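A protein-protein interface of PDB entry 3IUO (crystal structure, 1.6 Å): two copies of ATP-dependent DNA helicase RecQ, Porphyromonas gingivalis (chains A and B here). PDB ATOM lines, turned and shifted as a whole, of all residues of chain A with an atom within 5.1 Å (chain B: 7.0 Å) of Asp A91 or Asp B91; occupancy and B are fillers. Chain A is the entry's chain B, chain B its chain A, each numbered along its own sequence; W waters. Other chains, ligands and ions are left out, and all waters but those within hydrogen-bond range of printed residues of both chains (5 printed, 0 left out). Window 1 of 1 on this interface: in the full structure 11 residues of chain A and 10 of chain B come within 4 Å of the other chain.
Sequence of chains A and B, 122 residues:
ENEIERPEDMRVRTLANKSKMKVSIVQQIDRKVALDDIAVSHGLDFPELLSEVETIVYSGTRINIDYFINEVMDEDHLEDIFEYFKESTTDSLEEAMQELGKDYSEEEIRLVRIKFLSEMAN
The backbone carbonyl oxygen (O) of Thr A89 sits close to the side-chain sulfur (SD) of Met B120. The side-chain carboxylate (OD1) of Asp B91 lies within hydrogen-bond range of the side-chain hydroxyl (OG1) of Thr A90. OG1 of Thr B90 is in hydrogen-bond range of OD1 of Asp A91. The side-chain carboxylate (OD2) of Asp B91 is in hydrogen-bond range of the backbone NH (N) of Asp A91 (2.9 Å).
The guanidinium group of Arg B113 lies within hydrogen-bond range of the side-chain hydroxyl of Tyr B58. The backbone carbonyl oxygen of Phe A85 lies within hydrogen-bond range of the side-chain hydroxyl of Ser A88. The side-chain carboxylate of Asp B91 is in salt-bridge range of the guanidinium group of Arg B113 (2.9 Å). The backbone carbonyl oxygen (O) of Thr A90 sits at hydrogen-bond distance from the side-chain hydroxyl (OG) of Ser A88, at 3.4 Å. The backbone NH (N) of Ser B92 is in hydrogen-bond range of the side-chain hydroxyl (OG1) of Thr B90, 3.0 Å away. The side-chain hydroxyl (OG) of Ser B88 lies within hydrogen-bond range of the backbone carbonyl oxygen (O) of Thr B90 (3.1 Å).
CE of Met B120 touches O of Ser A88, 3.6 Å away. Thr A89 touches Tyr B58. Asp B91 touches Thr A89 (OD2 to O, 3.99 Å). O of Thr A89 touches CD2 of Leu B117, at 3.4 Å. Thr A90 touches Tyr B58. Arg B113 touches Thr A90. Arg A113 touches Thr B90. Leu A117 touches Thr B89 (CD2 to O, 3.4 Å).
Of chain B, only Thr B90 and Asp B91 come within 4 Å of Asp A91. Printed residues of chain A within 4 Å of Tyr B58: Thr A89 (3.9 Å) and Thr A90 (3.6 Å). Printed residues of chain A within 4 Å of Leu B117: Thr A89. Glu B94 touches none of the printed residues of chain A. The nearest printed residue of chain A that does not touch Asp B91 is Ser A92 (4.7 Å).
Hydrophobic or aromatic side chains of chain A that line the printed part of chain B: Leu A117. Of the 16 printed residues of chain B, 7 touch a printed residue of chain A. Printed residues of chain B that touch a printed residue of chain A: Tyr B58, Thr B89, Thr B90, Asp B91, Arg B113, Leu B117 and Met B120. Among the printed residues, 12 pairs touch across the chains. Among the printed residues, no Asp or Glu carboxylate lies within 4 Å of a Lys or Arg side-chain nitrogen of the other chain.
Thr A89 touches Leu B117, and with the chains exchanged Leu A117 touches Thr B89. Thr A90 touches Asp B91, and with the chains exchanged Asp A91 touches Thr B90. Thr A90 touches Arg B113, and with the chains exchanged Arg A113 touches Thr B90. Asp A91 touches its own counterpart, Asp B91. Positions printed for both chains: 85, 88, 89, 90, 91, 92, 93, 113 and 117.
Water W2 lies within hydrogen-bond range of OD2 of Asp B91 and O of Thr A89. Water W1 lies within hydrogen-bond range of the guanidinium group of Arg A113 (2.8 Å) and the side-chain hydroxyl of Thr B90 (3.3 Å). Water W3 lies within hydrogen-bond range of OD1 of Asp B91 (2.8 Å), OD1 of Asp A91 (2.9 Å), N of Ser B92 (3.2 Å) and N of Ser A92 (3.3 Å). Water W5 lies within hydrogen-bond range of NH2 of Arg B113 (2.8 Å), OH of Tyr B58 (3.0 Å) and OG1 of Thr A90 (3.2 Å). Water W4 bridges the backbone carbonyl oxygen of Thr B89 and the backbone carbonyl oxygen of Leu A117.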
ATOM      1  N   PHE A  85     -18.972  13.795  -2.619  1.00  0.00           N
ATOM      2  CA  PHE A  85     -20.123  14.248  -3.409  1.00  0.00           C
ATOM      3  C   PHE A  85     -20.770  13.130  -4.226  1.00  0.00           C
ATOM      4  O   PHE A  85     -22.014  13.023  -4.335  1.00  0.00           O
ATOM      5  CB  PHE A  85     -19.758  15.480  -4.260  1.00  0.00           C
ATOM      6  CG  PHE A  85     -19.709  16.752  -3.445  1.00  0.00           C
ATOM      7  CD1 PHE A  85     -20.901  17.283  -2.914  1.00  0.00           C
ATOM      8  CD2 PHE A  85     -18.496  17.372  -3.173  1.00  0.00           C
ATOM      9  CE1 PHE A  85     -20.866  18.438  -2.105  1.00  0.00           C
ATOM     10  CE2 PHE A  85     -18.445  18.542  -2.386  1.00  0.00           C
ATOM     11  CZ  PHE A  85     -19.633  19.078  -1.863  1.00  0.00           C
ATOM     12  N   SER A  88     -22.918  11.251  -1.861  1.00  0.00           N
ATOM     13  CA  SER A  88     -23.895  12.023  -1.084  1.00  0.00           C
ATOM     14  C   SER A  88     -25.304  11.922  -1.661  1.00  0.00           C
ATOM     15  O   SER A  88     -25.513  11.529  -2.827  1.00  0.00           O
ATOM     16  CB  SER A  88     -23.453  13.489  -1.039  1.00  0.00           C
ATOM     17  OG  SER A  88     -23.616  14.074  -2.325  1.00  0.00           O
ATOM     18  N   THR A  89     -26.281  12.275  -0.828  1.00  0.00           N
ATOM     19  CA  THR A  89     -27.670  12.385  -1.274  1.00  0.00           C
ATOM     20  C   THR A  89     -27.970  13.838  -1.584  1.00  0.00           C
ATOM     21  O   THR A  89     -28.527  14.127  -2.622  1.00  0.00           O
ATOM     22  CB  THR A  89     -28.633  11.784  -0.226  1.00  0.00           C
ATOM     23  OG1 THR A  89     -28.369  10.361  -0.104  1.00  0.00           O
ATOM     24  CG2 THR A  89     -30.090  11.995  -0.591  1.00  0.00           C
ATOM     25  N   THR A  90     -27.633  14.738  -0.670  1.00  0.00           N
ATOM     26  CA  THR A  90     -27.758  16.173  -0.963  1.00  0.00           C
ATOM     27  C   THR A  90     -26.391  16.767  -1.261  1.00  0.00           C
ATOM     28  O   THR A  90     -25.412  16.365  -0.646  1.00  0.00           O
ATOM     29  CB  THR A  90     -28.432  16.971   0.185  1.00  0.00           C
ATOM     30  OG1 THR A  90     -28.470  18.357  -0.175  1.00  0.00           O
ATOM     31  CG2 THR A  90     -27.697  16.820   1.502  1.00  0.00           C
ATOM     32  N   ASP A  91     -26.366  17.741  -2.186  1.00  0.00           N
ATOM     33  CA  ASP A  91     -25.137  18.451  -2.499  1.00  0.00           C
ATOM     34  C   ASP A  91     -24.847  19.617  -1.576  1.00  0.00           C
ATOM     35  O   ASP A  91     -23.842  20.305  -1.747  1.00  0.00           O
ATOM     36  CB  ASP A  91     -25.115  18.956  -3.965  1.00  0.00           C
ATOM     37  CG  ASP A  91     -26.251  19.964  -4.255  1.00  0.00           C
ATOM     38  OD1 ASP A  91     -26.279  21.061  -3.654  1.00  0.00           O
ATOM     39  OD2 ASP A  91     -27.122  19.627  -5.081  1.00  0.00           O
ATOM     40  N   SER A  92     -25.693  19.813  -0.569  1.00  0.00           N
ATOM     41  CA  SER A  92     -25.652  20.990   0.290  1.00  0.00           C
ATOM     42  C   SER A  92     -24.269  21.270   0.870  1.00  0.00           C
ATOM     43  O   SER A  92     -23.603  20.348   1.353  1.00  0.00           O
ATOM     44  CB  SER A  92     -26.709  20.791   1.383  1.00  0.00           C
ATOM     45  OG  SER A  92     -26.272  21.139   2.675  1.00  0.00           O
ATOM     46  N   LEU A  93     -23.838  22.546   0.846  1.00  0.00           N
ATOM     47  CA  LEU A  93     -22.562  22.890   1.467  1.00  0.00           C
ATOM     48  C   LEU A  93     -22.606  22.650   2.977  1.00  0.00           C
ATOM     49  O   LEU A  93     -21.631  22.189   3.554  1.00  0.00           O
ATOM     50  CB  LEU A  93     -22.165  24.354   1.196  1.00  0.00           C
ATOM     51  CG  LEU A  93     -20.809  24.825   1.755  1.00  0.00           C
ATOM     52  CD1 LEU A  93     -19.624  24.022   1.216  1.00  0.00           C
ATOM     53  CD2 LEU A  93     -20.551  26.319   1.526  1.00  0.00           C
ATOM     54  N   ARG A 113     -17.153  21.059  -5.108  1.00  0.00           N
ATOM     55  CA  ARG A 113     -18.608  21.011  -5.295  1.00  0.00           C
ATOM     56  C   ARG A 113     -18.979  21.664  -6.649  1.00  0.00           C
ATOM     57  O   ARG A 113     -19.839  21.149  -7.355  1.00  0.00           O
ATOM     58  CB  ARG A 113     -19.277  21.724  -4.123  1.00  0.00           C
ATOM     59  CG  ARG A 113     -20.806  21.771  -4.195  1.00  0.00           C
ATOM     60  CD  ARG A 113     -21.404  22.364  -2.946  1.00  0.00           C
ATOM     61  NE  ARG A 113     -22.870  22.486  -3.075  1.00  0.00           N
ATOM     62  CZ  ARG A 113     -23.474  23.557  -3.560  1.00  0.00           C
ATOM     63  NH1 ARG A 113     -22.751  24.594  -3.984  1.00  0.00           N
ATOM     64  NH2 ARG A 113     -24.794  23.574  -3.657  1.00  0.00           N
ATOM     65  N   LEU A 117     -20.975  19.517  -9.394  1.00  0.00           N
ATOM     66  CA  LEU A 117     -22.309  19.926  -9.908  1.00  0.00           C
ATOM     67  C   LEU A 117     -22.298  20.183 -11.393  1.00  0.00           C
ATOM     68  O   LEU A 117     -23.254  19.782 -12.105  1.00  0.00           O
ATOM     69  CB  LEU A 117     -22.805  21.175  -9.191  1.00  0.00           C
ATOM     70  CG  LEU A 117     -23.124  20.987  -7.713  1.00  0.00           C
ATOM     71  CD1 LEU A 117     -23.485  22.345  -7.107  1.00  0.00           C
ATOM     72  CD2 LEU A 117     -24.226  19.929  -7.443  1.00  0.00           C
ATOM     73  N   TYR B  58     -30.901  12.468   3.967  1.00  0.00           N
ATOM     74  CA  TYR B  58     -29.518  12.856   3.702  1.00  0.00           C
ATOM     75  C   TYR B  58     -28.532  11.764   4.043  1.00  0.00           C
ATOM     76  O   TYR B  58     -27.465  11.674   3.456  1.00  0.00           O
ATOM     77  CB  TYR B  58     -29.117  14.125   4.460  1.00  0.00           C
ATOM     78  CG  TYR B  58     -29.890  15.374   4.108  1.00  0.00           C
ATOM     79  CD1 TYR B  58     -30.687  15.484   2.929  1.00  0.00           C
ATOM     80  CD2 TYR B  58     -29.848  16.468   4.956  1.00  0.00           C
ATOM     81  CE1 TYR B  58     -31.420  16.637   2.666  1.00  0.00           C
ATOM     82  CE2 TYR B  58     -30.542  17.629   4.685  1.00  0.00           C
ATOM     83  CZ  TYR B  58     -31.340  17.711   3.543  1.00  0.00           C
ATOM     84  OH  TYR B  58     -32.000  18.867   3.316  1.00  0.00           O
ATOM     85  N   TYR B  84     -38.800  20.175 -11.917  1.00  0.00           N
ATOM     86  CA  TYR B  84     -37.808  21.171 -11.514  1.00  0.00           C
ATOM     87  C   TYR B  84     -36.596  20.464 -10.904  1.00  0.00           C
ATOM     88  O   TYR B  84     -35.486  20.759 -11.271  1.00  0.00           O
ATOM     89  CB  TYR B  84     -38.394  22.226 -10.546  1.00  0.00           C
ATOM     90  CG  TYR B  84     -37.278  22.967  -9.857  1.00  0.00           C
ATOM     91  CD1 TYR B  84     -36.695  24.077 -10.453  1.00  0.00           C
ATOM     92  CD2 TYR B  84     -36.736  22.482  -8.653  1.00  0.00           C
ATOM     93  CE1 TYR B  84     -35.624  24.734  -9.850  1.00  0.00           C
ATOM     94  CE2 TYR B  84     -35.676  23.116  -8.064  1.00  0.00           C
ATOM     95  CZ  TYR B  84     -35.122  24.235  -8.662  1.00  0.00           C
ATOM     96  OH  TYR B  84     -34.037  24.853  -8.075  1.00  0.00           O
ATOM     97  N   PHE B  85     -36.810  19.548  -9.957  1.00  0.00           N
ATOM     98  CA  PHE B  85     -35.642  18.878  -9.353  1.00  0.00           C
ATOM     99  C   PHE B  85     -34.865  18.013 -10.332  1.00  0.00           C
ATOM    100  O   PHE B  85     -33.598  18.000 -10.307  1.00  0.00           O
ATOM    101  CB  PHE B  85     -36.052  18.116  -8.105  1.00  0.00           C
ATOM    102  CG  PHE B  85     -36.290  19.029  -6.931  1.00  0.00           C
ATOM    103  CD1 PHE B  85     -35.206  19.683  -6.356  1.00  0.00           C
ATOM    104  CD2 PHE B  85     -37.577  19.241  -6.413  1.00  0.00           C
ATOM    105  CE1 PHE B  85     -35.387  20.565  -5.272  1.00  0.00           C
ATOM    106  CE2 PHE B  85     -37.745  20.116  -5.322  1.00  0.00           C
ATOM    107  CZ  PHE B  85     -36.628  20.788  -4.761  1.00  0.00           C
ATOM    108  N   SER B  88     -32.736  20.406 -12.332  1.00  0.00           N
ATOM    109  CA  SER B  88     -31.936  21.346 -11.554  1.00  0.00           C
ATOM    110  C   SER B  88     -30.479  20.903 -11.459  1.00  0.00           C
ATOM    111  O   SER B  88     -30.147  19.722 -11.627  1.00  0.00           O
ATOM    112  CB  SER B  88     -32.547  21.500 -10.138  1.00  0.00           C
ATOM    113  OG  SER B  88     -32.222  20.376  -9.363  1.00  0.00           O
ATOM    114  N   THR B  89     -29.597  21.857 -11.198  1.00  0.00           N
ATOM    115  CA  THR B  89     -28.188  21.526 -10.945  1.00  0.00           C
ATOM    116  C   THR B  89     -27.906  21.291  -9.475  1.00  0.00           C
ATOM    117  O   THR B  89     -27.194  20.339  -9.106  1.00  0.00           O
ATOM    118  CB  THR B  89     -27.292  22.639 -11.514  1.00  0.00           C
ATOM    119  OG1 THR B  89     -27.520  22.694 -12.929  1.00  0.00           O
ATOM    120  CG2 THR B  89     -25.786  22.399 -11.199  1.00  0.00           C
ATOM    121  N   THR B  90     -28.481  22.132  -8.634  1.00  0.00           N
ATOM    122  CA  THR B  90     -28.428  21.904  -7.180  1.00  0.00           C
ATOM    123  C   THR B  90     -29.792  21.547  -6.629  1.00  0.00           C
ATOM    124  O   THR B  90     -30.819  22.031  -7.149  1.00  0.00           O
ATOM    125  CB  THR B  90     -27.877  23.112  -6.403  1.00  0.00           C
ATOM    126  OG1 THR B  90     -27.983  22.848  -4.998  1.00  0.00           O
ATOM    127  CG2 THR B  90     -28.633  24.392  -6.688  1.00  0.00           C
ATOM    128  N   ASP B  91     -29.816  20.697  -5.584  1.00  0.00           N
ATOM    129  CA  ASP B  91     -31.074  20.345  -4.908  1.00  0.00           C
ATOM    130  C   ASP B  91     -31.506  21.355  -3.842  1.00  0.00           C
ATOM    131  O   ASP B  91     -32.552  21.177  -3.224  1.00  0.00           O
ATOM    132  CB  ASP B  91     -31.016  18.945  -4.284  1.00  0.00           C
ATOM    133  CG  ASP B  91     -29.974  18.818  -3.179  1.00  0.00           C
ATOM    134  OD1 ASP B  91     -30.068  19.517  -2.128  1.00  0.00           O
ATOM    135  OD2 ASP B  91     -29.036  18.016  -3.368  1.00  0.00           O
ATOM    136  N   SER B  92     -30.682  22.392  -3.662  1.00  0.00           N
ATOM    137  CA  SER B  92     -30.911  23.422  -2.634  1.00  0.00           C
ATOM    138  C   SER B  92     -32.359  23.884  -2.500  1.00  0.00           C
ATOM    139  O   SER B  92     -32.988  24.268  -3.486  1.00  0.00           O
ATOM    140  CB  SER B  92     -30.047  24.630  -3.036  1.00  0.00           C
ATOM    141  OG  SER B  92     -30.453  25.805  -2.436  1.00  0.00           O
ATOM    142  N   LEU B  93     -32.864  23.893  -1.254  1.00  0.00           N
ATOM    143  CA  LEU B  93     -34.166  24.447  -1.037  1.00  0.00           C
ATOM    144  C   LEU B  93     -34.193  25.940  -1.375  1.00  0.00           C
ATOM    145  O   LEU B  93     -35.193  26.421  -1.879  1.00  0.00           O
ATOM    146  CB  LEU B  93     -34.611  24.216   0.421  1.00  0.00           C
ATOM    147  CG  LEU B  93     -36.033  24.704   0.738  1.00  0.00           C
ATOM    148  CD1 LEU B  93     -37.079  23.956  -0.079  1.00  0.00           C
ATOM    149  CD2 LEU B  93     -36.238  24.471   2.187  1.00  0.00           C
ATOM    150  N   GLU B  94     -33.131  26.671  -1.059  1.00  0.00           N
ATOM    151  CA  GLU B  94     -33.084  28.115  -1.341  1.00  0.00           C
ATOM    152  C   GLU B  94     -33.239  28.369  -2.841  1.00  0.00           C
ATOM    153  O   GLU B  94     -33.992  29.260  -3.285  1.00  0.00           O
ATOM    154  CB  GLU B  94     -31.765  28.728  -0.831  1.00  0.00           C
ATOM    155  CG  GLU B  94     -31.619  30.228  -1.007  1.00  0.00           C
ATOM    156  CD  GLU B  94     -30.336  30.799  -0.384  1.00  0.00           C
ATOM    157  OE1 GLU B  94     -29.941  30.371   0.725  1.00  0.00           O
ATOM    158  OE2 GLU B  94     -29.740  31.701  -0.999  1.00  0.00           O
ATOM    159  N   GLU B  95     -32.519  27.591  -3.643  1.00  0.00           N
ATOM    160  CA  GLU B  95     -32.674  27.723  -5.095  1.00  0.00           C
ATOM    161  C   GLU B  95     -34.058  27.344  -5.580  1.00  0.00           C
ATOM    162  O   GLU B  95     -34.611  28.017  -6.483  1.00  0.00           O
ATOM    163  CB  GLU B  95     -31.600  26.915  -5.837  1.00  0.00           C
ATOM    164  CG  GLU B  95     -30.179  27.482  -5.636  1.00  0.00           C
ATOM    165  CD  GLU B  95     -29.990  28.946  -6.008  1.00  0.00           C
ATOM    166  OE1 GLU B  95     -30.345  29.299  -7.158  1.00  0.00           O
ATOM    167  OE2 GLU B  95     -29.428  29.721  -5.173  1.00  0.00           O
ATOM    168  N   ALA B  96     -34.614  26.266  -5.010  1.00  0.00           N
ATOM    169  CA  ALA B  96     -35.961  25.825  -5.381  1.00  0.00           C
ATOM    170  C   ALA B  96     -37.006  26.883  -5.024  1.00  0.00           C
ATOM    171  O   ALA B  96     -37.930  27.159  -5.806  1.00  0.00           O
ATOM    172  CB  ALA B  96     -36.280  24.482  -4.730  1.00  0.00           C
ATOM    173  N   ARG B 113     -39.132  17.432  -2.747  1.00  0.00           N
ATOM    174  CA  ARG B 113     -37.679  17.293  -2.646  1.00  0.00           C
ATOM    175  C   ARG B 113     -37.255  16.043  -1.907  1.00  0.00           C
ATOM    176  O   ARG B 113     -36.309  15.379  -2.329  1.00  0.00           O
ATOM    177  CB  ARG B 113     -37.073  18.549  -1.997  1.00  0.00           C
ATOM    178  CG  ARG B 113     -35.577  18.480  -1.805  1.00  0.00           C
ATOM    179  CD  ARG B 113     -35.095  19.848  -1.312  1.00  0.00           C
ATOM    180  NE  ARG B 113     -33.654  19.868  -1.080  1.00  0.00           N
ATOM    181  CZ  ARG B 113     -33.077  19.563   0.076  1.00  0.00           C
ATOM    182  NH1 ARG B 113     -33.826  19.237   1.137  1.00  0.00           N
ATOM    183  NH2 ARG B 113     -31.767  19.587   0.188  1.00  0.00           N
ATOM    184  N   PHE B 116     -37.738  13.190  -4.341  1.00  0.00           N
ATOM    185  CA  PHE B 116     -36.700  13.240  -5.344  1.00  0.00           C
ATOM    186  C   PHE B 116     -35.349  12.711  -4.807  1.00  0.00           C
ATOM    187  O   PHE B 116     -34.705  11.852  -5.433  1.00  0.00           O
ATOM    188  CB  PHE B 116     -36.566  14.666  -5.902  1.00  0.00           C
ATOM    189  CG  PHE B 116     -35.396  14.835  -6.809  1.00  0.00           C
ATOM    190  CD1 PHE B 116     -35.465  14.416  -8.135  1.00  0.00           C
ATOM    191  CD2 PHE B 116     -34.213  15.378  -6.327  1.00  0.00           C
ATOM    192  CE1 PHE B 116     -34.364  14.546  -8.982  1.00  0.00           C
ATOM    193  CE2 PHE B 116     -33.121  15.533  -7.166  1.00  0.00           C
ATOM    194  CZ  PHE B 116     -33.189  15.110  -8.489  1.00  0.00           C
ATOM    195  N   LEU B 117     -34.935  13.233  -3.650  1.00  0.00           N
ATOM    196  CA  LEU B 117     -33.651  12.803  -3.078  1.00  0.00           C
ATOM    197  C   LEU B 117     -33.668  11.334  -2.693  1.00  0.00           C
ATOM    198  O   LEU B 117     -32.662  10.612  -2.881  1.00  0.00           O
ATOM    199  CB  LEU B 117     -33.298  13.675  -1.881  1.00  0.00           C
ATOM    200  CG  LEU B 117     -32.968  15.140  -2.169  1.00  0.00           C
ATOM    201  CD1 LEU B 117     -32.770  15.860  -0.842  1.00  0.00           C
ATOM    202  CD2 LEU B 117     -31.716  15.308  -3.074  1.00  0.00           C
ATOM    203  N   MET B 120     -32.881   8.834  -5.662  1.00  0.00           N
ATOM    204  CA  MET B 120     -31.489   8.655  -6.118  1.00  0.00           C
ATOM    205  C   MET B 120     -30.959   7.228  -5.932  1.00  0.00           C
ATOM    206  O   MET B 120     -31.072   6.633  -4.851  1.00  0.00           O
ATOM    207  CB  MET B 120     -30.582   9.652  -5.418  1.00  0.00           C
ATOM    208  CG  MET B 120     -30.943  11.081  -5.741  1.00  0.00           C
ATOM    209  SD  MET B 120     -30.010  12.325  -4.560  1.00  0.00           S
ATOM    210  CE  MET B 120     -28.174  12.054  -5.252  1.00  0.00           C
HETATM  211  O   HOH W   1     -26.924  25.347  -3.151  1.00  0.00           O
HETATM  212  O   HOH W   2     -28.560  16.224  -5.005  1.00  0.00           O
HETATM  213  O   HOH W   3     -28.276  21.651  -1.645  1.00  0.00           O
HETATM  214  O   HOH W   4     -25.424  18.372 -10.149  1.00  0.00           O
HETATM  215  O   HOH W   5     -29.733  20.371   2.001  1.00  0.00           O
